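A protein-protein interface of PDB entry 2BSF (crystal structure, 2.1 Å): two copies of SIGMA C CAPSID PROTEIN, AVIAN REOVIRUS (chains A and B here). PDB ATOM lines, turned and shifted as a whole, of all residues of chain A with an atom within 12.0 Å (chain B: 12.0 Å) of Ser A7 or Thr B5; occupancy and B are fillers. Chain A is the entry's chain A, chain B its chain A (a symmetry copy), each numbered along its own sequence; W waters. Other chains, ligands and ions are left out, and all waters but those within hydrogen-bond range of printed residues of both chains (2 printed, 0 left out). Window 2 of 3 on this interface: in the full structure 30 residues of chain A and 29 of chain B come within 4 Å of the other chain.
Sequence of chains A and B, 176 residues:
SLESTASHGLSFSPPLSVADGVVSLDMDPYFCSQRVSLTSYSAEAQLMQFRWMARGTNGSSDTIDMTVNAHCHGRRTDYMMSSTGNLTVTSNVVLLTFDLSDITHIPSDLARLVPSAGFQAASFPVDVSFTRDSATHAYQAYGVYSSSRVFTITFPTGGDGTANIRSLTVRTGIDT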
ATOM      1  N   SER A   1     -19.432   9.721  12.117  1.00  0.00           N
ATOM      2  CA  SER A   1     -19.959   8.526  12.851  1.00  0.00           C
ATOM      3  C   SER A   1     -20.375   7.327  11.983  1.00  0.00           C
ATOM      4  O   SER A   1     -21.454   7.323  11.339  1.00  0.00           O
ATOM      5  CB  SER A   1     -21.084   8.919  13.817  1.00  0.00           C
ATOM      6  OG  SER A   1     -20.644   8.833  15.162  1.00  0.00           O
ATOM      7  N   LEU A   2     -19.424   6.392  11.912  1.00  0.00           N
ATOM      8  CA  LEU A   2     -19.534   4.924  11.667  1.00  0.00           C
ATOM      9  C   LEU A   2     -20.382   4.278  10.556  1.00  0.00           C
ATOM     10  O   LEU A   2     -20.142   3.116  10.187  1.00  0.00           O
ATOM     11  CB  LEU A   2     -19.597   4.118  12.988  1.00  0.00           C
ATOM     12  CG  LEU A   2     -18.248   3.859  13.691  1.00  0.00           C
ATOM     13  CD1 LEU A   2     -17.295   5.099  13.704  1.00  0.00           C
ATOM     14  CD2 LEU A   2     -18.384   3.267  15.098  1.00  0.00           C
ATOM     15  N   GLU A   3     -21.358   5.016  10.034  1.00  0.00           N
ATOM     16  CA  GLU A   3     -22.133   4.539   8.899  1.00  0.00           C
ATOM     17  C   GLU A   3     -21.379   4.771   7.605  1.00  0.00           C
ATOM     18  O   GLU A   3     -20.511   5.650   7.520  1.00  0.00           O
ATOM     19  CB  GLU A   3     -23.449   5.287   8.840  1.00  0.00           C
ATOM     20  CG  GLU A   3     -24.459   4.698   9.772  1.00  0.00           C
ATOM     21  CD  GLU A   3     -25.607   5.623  10.018  1.00  0.00           C
ATOM     22  OE1 GLU A   3     -25.788   6.625   9.284  1.00  0.00           O
ATOM     23  OE2 GLU A   3     -26.344   5.335  10.958  1.00  0.00           O
ATOM     24  N   SER A   4     -21.713   3.970   6.604  1.00  0.00           N
ATOM     25  CA  SER A   4     -21.309   4.226   5.247  1.00  0.00           C
ATOM     26  C   SER A   4     -22.556   4.685   4.474  1.00  0.00           C
ATOM     27  O   SER A   4     -23.659   4.744   5.039  1.00  0.00           O
ATOM     28  CB  SER A   4     -20.658   2.980   4.629  1.00  0.00           C
ATOM     29  OG  SER A   4     -21.612   2.111   4.054  1.00  0.00           O
ATOM     30  N   THR A   5     -22.375   5.033   3.202  1.00  0.00           N
ATOM     31  CA  THR A   5     -23.493   5.430   2.351  1.00  0.00           C
ATOM     32  C   THR A   5     -24.456   4.249   2.155  1.00  0.00           C
ATOM     33  O   THR A   5     -25.599   4.453   1.763  1.00  0.00           O
ATOM     34  CB  THR A   5     -23.024   5.973   0.960  1.00  0.00           C
ATOM     35  OG1 THR A   5     -22.172   5.006   0.344  1.00  0.00           O
ATOM     36  CG2 THR A   5     -22.277   7.289   1.079  1.00  0.00           C
ATOM     37  N   ALA A   6     -23.990   3.031   2.454  1.00  0.00           N
ATOM     38  CA  ALA A   6     -24.809   1.805   2.378  1.00  0.00           C
ATOM     39  C   ALA A   6     -25.657   1.436   3.614  1.00  0.00           C
ATOM     40  O   ALA A   6     -26.601   0.643   3.502  1.00  0.00           O
ATOM     41  CB  ALA A   6     -23.921   0.626   2.015  1.00  0.00           C
ATOM     42  N   SER A   7     -25.298   1.978   4.780  1.00  0.00           N
ATOM     43  CA  SER A   7     -25.927   1.624   6.065  1.00  0.00           C
ATOM     44  C   SER A   7     -27.460   1.709   6.070  1.00  0.00           C
ATOM     45  O   SER A   7     -28.142   0.765   6.485  1.00  0.00           O
ATOM     46  CB  SER A   7     -25.379   2.510   7.191  1.00  0.00           C
ATOM     47  OG  SER A   7     -24.003   2.271   7.350  1.00  0.00           O
ATOM     48  N   HIS A   8     -27.984   2.850   5.634  1.00  0.00           N
ATOM     49  CA  HIS A   8     -29.428   3.067   5.655  1.00  0.00           C
ATOM     50  C   HIS A   8     -30.243   2.218   4.688  1.00  0.00           C
ATOM     51  O   HIS A   8     -31.450   2.049   4.891  1.00  0.00           O
ATOM     52  CB  HIS A   8     -29.742   4.530   5.501  1.00  0.00           C
ATOM     53  CG  HIS A   8     -29.453   5.312   6.736  1.00  0.00           C
ATOM     54  ND1 HIS A   8     -29.785   6.637   6.867  1.00  0.00           N
ATOM     55  CD2 HIS A   8     -28.869   4.946   7.904  1.00  0.00           C
ATOM     56  CE1 HIS A   8     -29.405   7.067   8.056  1.00  0.00           C
ATOM     57  NE2 HIS A   8     -28.841   6.060   8.701  1.00  0.00           N
ATOM     58  N   GLY A   9     -29.585   1.681   3.657  1.00  0.00           N
ATOM     59  CA  GLY A   9     -30.226   0.728   2.749  1.00  0.00           C
ATOM     60  C   GLY A   9     -31.178   1.342   1.723  1.00  0.00           C
ATOM     61  O   GLY A   9     -31.581   2.519   1.824  1.00  0.00           O
ATOM     62  N   LEU A  10     -31.538   0.529   0.733  1.00  0.00           N
ATOM     63  CA  LEU A  10     -32.424   0.963  -0.338  1.00  0.00           C
ATOM     64  C   LEU A  10     -33.835   0.414  -0.138  1.00  0.00           C
ATOM     65  O   LEU A  10     -34.049  -0.731   0.305  1.00  0.00           O
ATOM     66  CB  LEU A  10     -31.883   0.579  -1.714  1.00  0.00           C
ATOM     67  CG  LEU A  10     -30.441   0.913  -2.095  1.00  0.00           C
ATOM     68  CD1 LEU A  10     -29.528  -0.245  -1.690  1.00  0.00           C
ATOM     69  CD2 LEU A  10     -30.304   1.137  -3.562  1.00  0.00           C
ATOM     70  N   SER A  11     -34.788   1.270  -0.460  1.00  0.00           N
ATOM     71  CA  SER A  11     -36.186   0.933  -0.477  1.00  0.00           C
ATOM     72  C   SER A  11     -36.589   0.775  -1.983  1.00  0.00           C
ATOM     73  O   SER A  11     -35.987   1.411  -2.864  1.00  0.00           O
ATOM     74  CB  SER A  11     -36.943   2.065   0.225  1.00  0.00           C
ATOM     75  OG  SER A  11     -38.345   1.895   0.196  1.00  0.00           O
ATOM     76  N   PHE A  12     -37.556  -0.099  -2.264  1.00  0.00           N
ATOM     77  CA  PHE A  12     -37.994  -0.362  -3.645  1.00  0.00           C
ATOM     78  C   PHE A  12     -39.486  -0.140  -3.812  1.00  0.00           C
ATOM     79  O   PHE A  12     -40.304  -0.820  -3.187  1.00  0.00           O
ATOM     80  CB  PHE A  12     -37.569  -1.756  -4.098  1.00  0.00           C
ATOM     81  CG  PHE A  12     -36.091  -1.892  -4.237  1.00  0.00           C
ATOM     82  CD1 PHE A  12     -35.458  -1.545  -5.421  1.00  0.00           C
ATOM     83  CD2 PHE A  12     -35.314  -2.307  -3.150  1.00  0.00           C
ATOM     84  CE1 PHE A  12     -34.070  -1.635  -5.538  1.00  0.00           C
ATOM     85  CE2 PHE A  12     -33.942  -2.398  -3.254  1.00  0.00           C
ATOM     86  CZ  PHE A  12     -33.312  -2.056  -4.441  1.00  0.00           C
ATOM     87  N   VAL A  18     -38.281  -5.966  -3.310  1.00  0.00           N
ATOM     88  CA  VAL A  18     -37.164  -6.799  -2.806  1.00  0.00           C
ATOM     89  C   VAL A  18     -37.694  -7.891  -1.852  1.00  0.00           C
ATOM     90  O   VAL A  18     -38.627  -7.654  -1.081  1.00  0.00           O
ATOM     91  CB  VAL A  18     -35.982  -5.939  -2.183  1.00  0.00           C
ATOM     92  CG1 VAL A  18     -36.455  -5.080  -1.003  1.00  0.00           C
ATOM     93  CG2 VAL A  18     -34.755  -6.839  -1.777  1.00  0.00           C
ATOM     94  N   ALA A  19     -37.122  -9.089  -1.940  1.00  0.00           N
ATOM     95  CA  ALA A  19     -37.414 -10.161  -1.008  1.00  0.00           C
ATOM     96  C   ALA A  19     -36.141 -10.959  -0.823  1.00  0.00           C
ATOM     97  O   ALA A  19     -35.610 -11.488  -1.796  1.00  0.00           O
ATOM     98  CB  ALA A  19     -38.522 -11.061  -1.553  1.00  0.00           C
ATOM     99  N   ASP A  20     -35.642 -11.042   0.415  1.00  0.00           N
ATOM    100  CA  ASP A  20     -34.455 -11.863   0.718  1.00  0.00           C
ATOM    101  C   ASP A  20     -33.225 -11.374  -0.020  1.00  0.00           C
ATOM    102  O   ASP A  20     -32.419 -12.183  -0.469  1.00  0.00           O
ATOM    103  CB  ASP A  20     -34.674 -13.327   0.313  1.00  0.00           C
ATOM    104  CG  ASP A  20     -35.489 -14.119   1.319  1.00  0.00           C
ATOM    105  OD1 ASP A  20     -36.236 -13.524   2.131  1.00  0.00           O
ATOM    106  OD2 ASP A  20     -35.380 -15.365   1.279  1.00  0.00           O
ATOM    107  N   GLY A  21     -33.092 -10.058  -0.154  1.00  0.00           N
ATOM    108  CA  GLY A  21     -32.005  -9.443  -0.922  1.00  0.00           C
ATOM    109  C   GLY A  21     -32.081  -9.658  -2.432  1.00  0.00           C
ATOM    110  O   GLY A  21     -31.110  -9.395  -3.141  1.00  0.00           O
ATOM    111  N   VAL A  22     -33.215 -10.163  -2.926  1.00  0.00           N
ATOM    112  CA  VAL A  22     -33.391 -10.336  -4.374  1.00  0.00           C
ATOM    113  C   VAL A  22     -34.404  -9.301  -4.882  1.00  0.00           C
ATOM    114  O   VAL A  22     -35.551  -9.273  -4.447  1.00  0.00           O
ATOM    115  CB  VAL A  22     -33.831 -11.765  -4.769  1.00  0.00           C
ATOM    116  CG1 VAL A  22     -34.066 -11.826  -6.259  1.00  0.00           C
ATOM    117  CG2 VAL A  22     -32.775 -12.803  -4.364  1.00  0.00           C
ATOM    118  N   VAL A  23     -33.939  -8.427  -5.768  1.00  0.00           N
ATOM    119  CA  VAL A  23     -34.753  -7.347  -6.296  1.00  0.00           C
ATOM    120  C   VAL A  23     -35.384  -7.791  -7.623  1.00  0.00           C
ATOM    121  O   VAL A  23     -34.690  -8.291  -8.517  1.00  0.00           O
ATOM    122  CB  VAL A  23     -33.931  -6.077  -6.490  1.00  0.00           C
ATOM    123  CG1 VAL A  23     -34.835  -4.922  -6.962  1.00  0.00           C
ATOM    124  CG2 VAL A  23     -33.210  -5.716  -5.190  1.00  0.00           C
ATOM    125  N   SER B   1     -22.459  -9.442  15.497  1.00  0.00           N
ATOM    126  CA  SER B   1     -21.234  -9.600  14.652  1.00  0.00           C
ATOM    127  C   SER B   1     -21.218  -8.814  13.329  1.00  0.00           C
ATOM    128  O   SER B   1     -21.876  -9.196  12.329  1.00  0.00           O
ATOM    129  CB  SER B   1     -20.910 -11.081  14.413  1.00  0.00           C
ATOM    130  OG  SER B   1     -19.756 -11.465  15.142  1.00  0.00           O
ATOM    131  N   LEU B   2     -20.545  -7.666  13.425  1.00  0.00           N
ATOM    132  CA  LEU B   2     -19.836  -6.876  12.374  1.00  0.00           C
ATOM    133  C   LEU B   2     -20.417  -6.529  10.992  1.00  0.00           C
ATOM    134  O   LEU B   2     -19.941  -5.587  10.336  1.00  0.00           O
ATOM    135  CB  LEU B   2     -18.330  -7.230  12.300  1.00  0.00           C
ATOM    136  CG  LEU B   2     -17.422  -6.565  13.356  1.00  0.00           C
ATOM    137  CD1 LEU B   2     -18.038  -6.545  14.793  1.00  0.00           C
ATOM    138  CD2 LEU B   2     -15.995  -7.123  13.386  1.00  0.00           C
ATOM    139  N   GLU B   3     -21.428  -7.276  10.556  1.00  0.00           N
ATOM    140  CA  GLU B   3     -22.121  -6.951   9.319  1.00  0.00           C
ATOM    141  C   GLU B   3     -23.143  -5.857   9.555  1.00  0.00           C
ATOM    142  O   GLU B   3     -23.621  -5.660  10.679  1.00  0.00           O
ATOM    143  CB  GLU B   3     -22.834  -8.185   8.803  1.00  0.00           C
ATOM    144  CG  GLU B   3     -21.908  -9.079   8.044  1.00  0.00           C
ATOM    145  CD  GLU B   3     -22.470 -10.450   7.861  1.00  0.00           C
ATOM    146  OE1 GLU B   3     -23.685 -10.677   8.083  1.00  0.00           O
ATOM    147  OE2 GLU B   3     -21.683 -11.315   7.483  1.00  0.00           O
ATOM    148  N   SER B   4     -23.464  -5.142   8.485  1.00  0.00           N
ATOM    149  CA  SER B   4     -24.603  -4.264   8.462  1.00  0.00           C
ATOM    150  C   SER B   4     -25.673  -4.920   7.576  1.00  0.00           C
ATOM    151  O   SER B   4     -25.446  -6.003   7.013  1.00  0.00           O
ATOM    152  CB  SER B   4     -24.202  -2.868   7.965  1.00  0.00           C
ATOM    153  OG  SER B   4     -24.250  -2.770   6.557  1.00  0.00           O
ATOM    154  N   THR B   5     -26.839  -4.285   7.477  1.00  0.00           N
ATOM    155  CA  THR B   5     -27.910  -4.781   6.619  1.00  0.00           C
ATOM    156  C   THR B   5     -27.475  -4.739   5.146  1.00  0.00           C
ATOM    157  O   THR B   5     -28.078  -5.404   4.312  1.00  0.00           O
ATOM    158  CB  THR B   5     -29.244  -3.983   6.804  1.00  0.00           C
ATOM    159  OG1 THR B   5     -28.984  -2.591   6.620  1.00  0.00           O
ATOM    160  CG2 THR B   5     -29.857  -4.197   8.176  1.00  0.00           C
ATOM    161  N   ALA B   6     -26.416  -3.976   4.850  1.00  0.00           N
ATOM    162  CA  ALA B   6     -25.837  -3.879   3.495  1.00  0.00           C
ATOM    163  C   ALA B   6     -24.789  -4.937   3.089  1.00  0.00           C
ATOM    164  O   ALA B   6     -24.526  -5.122   1.894  1.00  0.00           O
ATOM    165  CB  ALA B   6     -25.246  -2.493   3.296  1.00  0.00           C
ATOM    166  N   SER B   7     -24.175  -5.594   4.076  1.00  0.00           N
ATOM    167  CA  SER B   7     -23.067  -6.539   3.855  1.00  0.00           C
ATOM    168  C   SER B   7     -23.351  -7.623   2.806  1.00  0.00           C
ATOM    169  O   SER B   7     -22.550  -7.838   1.889  1.00  0.00           O
ATOM    170  CB  SER B   7     -22.668  -7.216   5.171  1.00  0.00           C
ATOM    171  OG  SER B   7     -22.186  -6.251   6.071  1.00  0.00           O
ATOM    172  N   HIS B   8     -24.476  -8.311   2.967  1.00  0.00           N
ATOM    173  CA  HIS B   8     -24.817  -9.410   2.067  1.00  0.00           C
ATOM    174  C   HIS B   8     -25.157  -9.017   0.635  1.00  0.00           C
ATOM    175  O   HIS B   8     -25.081  -9.860  -0.264  1.00  0.00           O
ATOM    176  CB  HIS B   8     -25.894 -10.269   2.671  1.00  0.00           C
ATOM    177  CG  HIS B   8     -25.387 -11.130   3.776  1.00  0.00           C
ATOM    178  ND1 HIS B   8     -26.162 -12.088   4.383  1.00  0.00           N
ATOM    179  CD2 HIS B   8     -24.174 -11.182   4.379  1.00  0.00           C
ATOM    180  CE1 HIS B   8     -25.459 -12.686   5.326  1.00  0.00           C
ATOM    181  NE2 HIS B   8     -24.250 -12.149   5.346  1.00  0.00           N
ATOM    182  N   GLY B   9     -25.512  -7.746   0.429  1.00  0.00           N
ATOM    183  CA  GLY B   9     -25.715  -7.215  -0.921  1.00  0.00           C
ATOM    184  C   GLY B   9     -27.031  -7.613  -1.589  1.00  0.00           C
ATOM    185  O   GLY B   9     -27.747  -8.527  -1.134  1.00  0.00           O
ATOM    186  N   LEU B  10     -27.340  -6.916  -2.680  1.00  0.00           N
ATOM    187  CA  LEU B  10     -28.568  -7.155  -3.425  1.00  0.00           C
ATOM    188  C   LEU B  10     -28.290  -7.946  -4.702  1.00  0.00           C
ATOM    189  O   LEU B  10     -27.270  -7.759  -5.393  1.00  0.00           O
ATOM    190  CB  LEU B  10     -29.302  -5.853  -3.743  1.00  0.00           C
ATOM    191  CG  LEU B  10     -29.581  -4.836  -2.636  1.00  0.00           C
ATOM    192  CD1 LEU B  10     -28.409  -3.859  -2.538  1.00  0.00           C
ATOM    193  CD2 LEU B  10     -30.826  -4.063  -2.908  1.00  0.00           C
ATOM    194  N   SER B  11     -29.217  -8.845  -4.981  1.00  0.00           N
ATOM    195  CA  SER B  11     -29.234  -9.615  -6.195  1.00  0.00           C
ATOM    196  C   SER B  11     -30.354  -8.996  -7.100  1.00  0.00           C
ATOM    197  O   SER B  11     -31.334  -8.429  -6.587  1.00  0.00           O
ATOM    198  CB  SER B  11     -29.517 -11.072  -5.814  1.00  0.00           C
ATOM    199  OG  SER B  11     -29.648 -11.923  -6.935  1.00  0.00           O
ATOM    200  N   PHE B  12     -30.175  -9.064  -8.420  1.00  0.00           N
ATOM    201  CA  PHE B  12     -31.139  -8.483  -9.370  1.00  0.00           C
ATOM    202  C   PHE B  12     -31.634  -9.516 -10.366  1.00  0.00           C
ATOM    203  O   PHE B  12     -30.857 -10.069 -11.149  1.00  0.00           O
ATOM    204  CB  PHE B  12     -30.554  -7.256 -10.062  1.00  0.00           C
ATOM    205  CG  PHE B  12     -30.349  -6.112  -9.129  1.00  0.00           C
ATOM    206  CD1 PHE B  12     -31.376  -5.215  -8.873  1.00  0.00           C
ATOM    207  CD2 PHE B  12     -29.136  -5.965  -8.446  1.00  0.00           C
ATOM    208  CE1 PHE B  12     -31.196  -4.166  -7.970  1.00  0.00           C
ATOM    209  CE2 PHE B  12     -28.950  -4.932  -7.550  1.00  0.00           C
ATOM    210  CZ  PHE B  12     -29.976  -4.035  -7.301  1.00  0.00           C
HETATM  211  O   HOH W   1     -28.460 -11.083  -2.565  1.00  0.00           O
HETATM  212  O   HOH W   2     -28.224  -1.245   4.645  1.00  0.00           O
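No residue of chain B comes within 4 Å of Glu A3. No residue of chain B comes within 4 Å of Thr A5. Of chain B, only Ala B6 comes within 4 Å of Ala A6. Printed residues of chain B within 4 Å of Ser A7: Thr B5 (3.5 Å). No residue of chain B comes within 4 Å of His A8. No residue of chain B comes within 4 Å of Gly A9. Printed residues of chain B within 4 Å of Leu A10: Leu B10. Of the printed residues of chain B, Phe A12 touches Leu B10. Ser B1 touches none of the printed residues of chain A. No residue of chain A comes within 4 Å of Ser B4. Thr B5 touches just one residue of chain A: Ser A7 (3.5 Å). Ala B6 touches one residue of chain A. Ser B7 touches none of the printed residues of chain A. Printed residues of chain A within 4 Å of Ser B11: Gly A21, Val A22 and Val A23. The nearest residue of chain A that does not touch Thr B5 is Ala A6 (5.1 Å).
O of Ser A7 is in hydrogen-bond range of OG1 of Thr B5, 3.5 Å away. The backbone carbonyl oxygen (O) of Gly A21 is in hydrogen-bond range of the backbone NH (N) of Ser B11 (2.7 Å). N of Val A23 is in hydrogen-bond range of O of Ser B11 (2.7 Å).
Ala A6 touches its own counterpart, Ala B6. Ser A7 touches Thr B5, but with the chains exchanged Thr A5 does not touch Ser B7 (10.0 Å). Leu B10 touches its own counterpart, Leu A10. Phe A12 touches Leu B10, but with the chains exchanged Leu A10 does not touch Phe B12 (6.4 Å). Of the 10 pairs that touch across the chains among the printed residues, 2 have their exchanged pair printed and touching as well.
Ala A6 touches Ala B6 (O to CB, 3.4 Å). Leu B10 touches Leu A10 (CD1 to CD1, 3.9 Å). Leu B10 touches Phe A12. O of Gly A21 touches CA of Leu B10, at 3.4 Å. Ser B11 touches Val A22 (O to CA, 3.6 Å). CD2 of Leu B10 touches CG2 of Val A23, at 3.7 Å. Val A23 touches Phe B12.
Water W2 lies within hydrogen-bond range of OG1 of Thr B5 (2.5 Å), O of Ser A7 (2.7 Å), O of Ala A6 (2.7 Å), N of Ala B6 (3.3 Å) and N of Gly A9 (3.4 Å). Water W1 lies within hydrogen-bond range of O of Gly B9, O of Gly A21 and N of Ser B11.
The side-chain hydroxyl of Ser A4 sits close to the backbone NH of Ala A6 (3.0 Å). N of Ser A4 sits at hydrogen-bond distance from OG of Ser A7 (2.9 Å). The backbone NH (N) of Ala B6 sits close to the side-chain hydroxyl (OG) of Ser B4.
Among the printed residues, no Asp or Glu carboxylate lies within 4 Å of a Lys or Arg side-chain nitrogen of the other chain.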
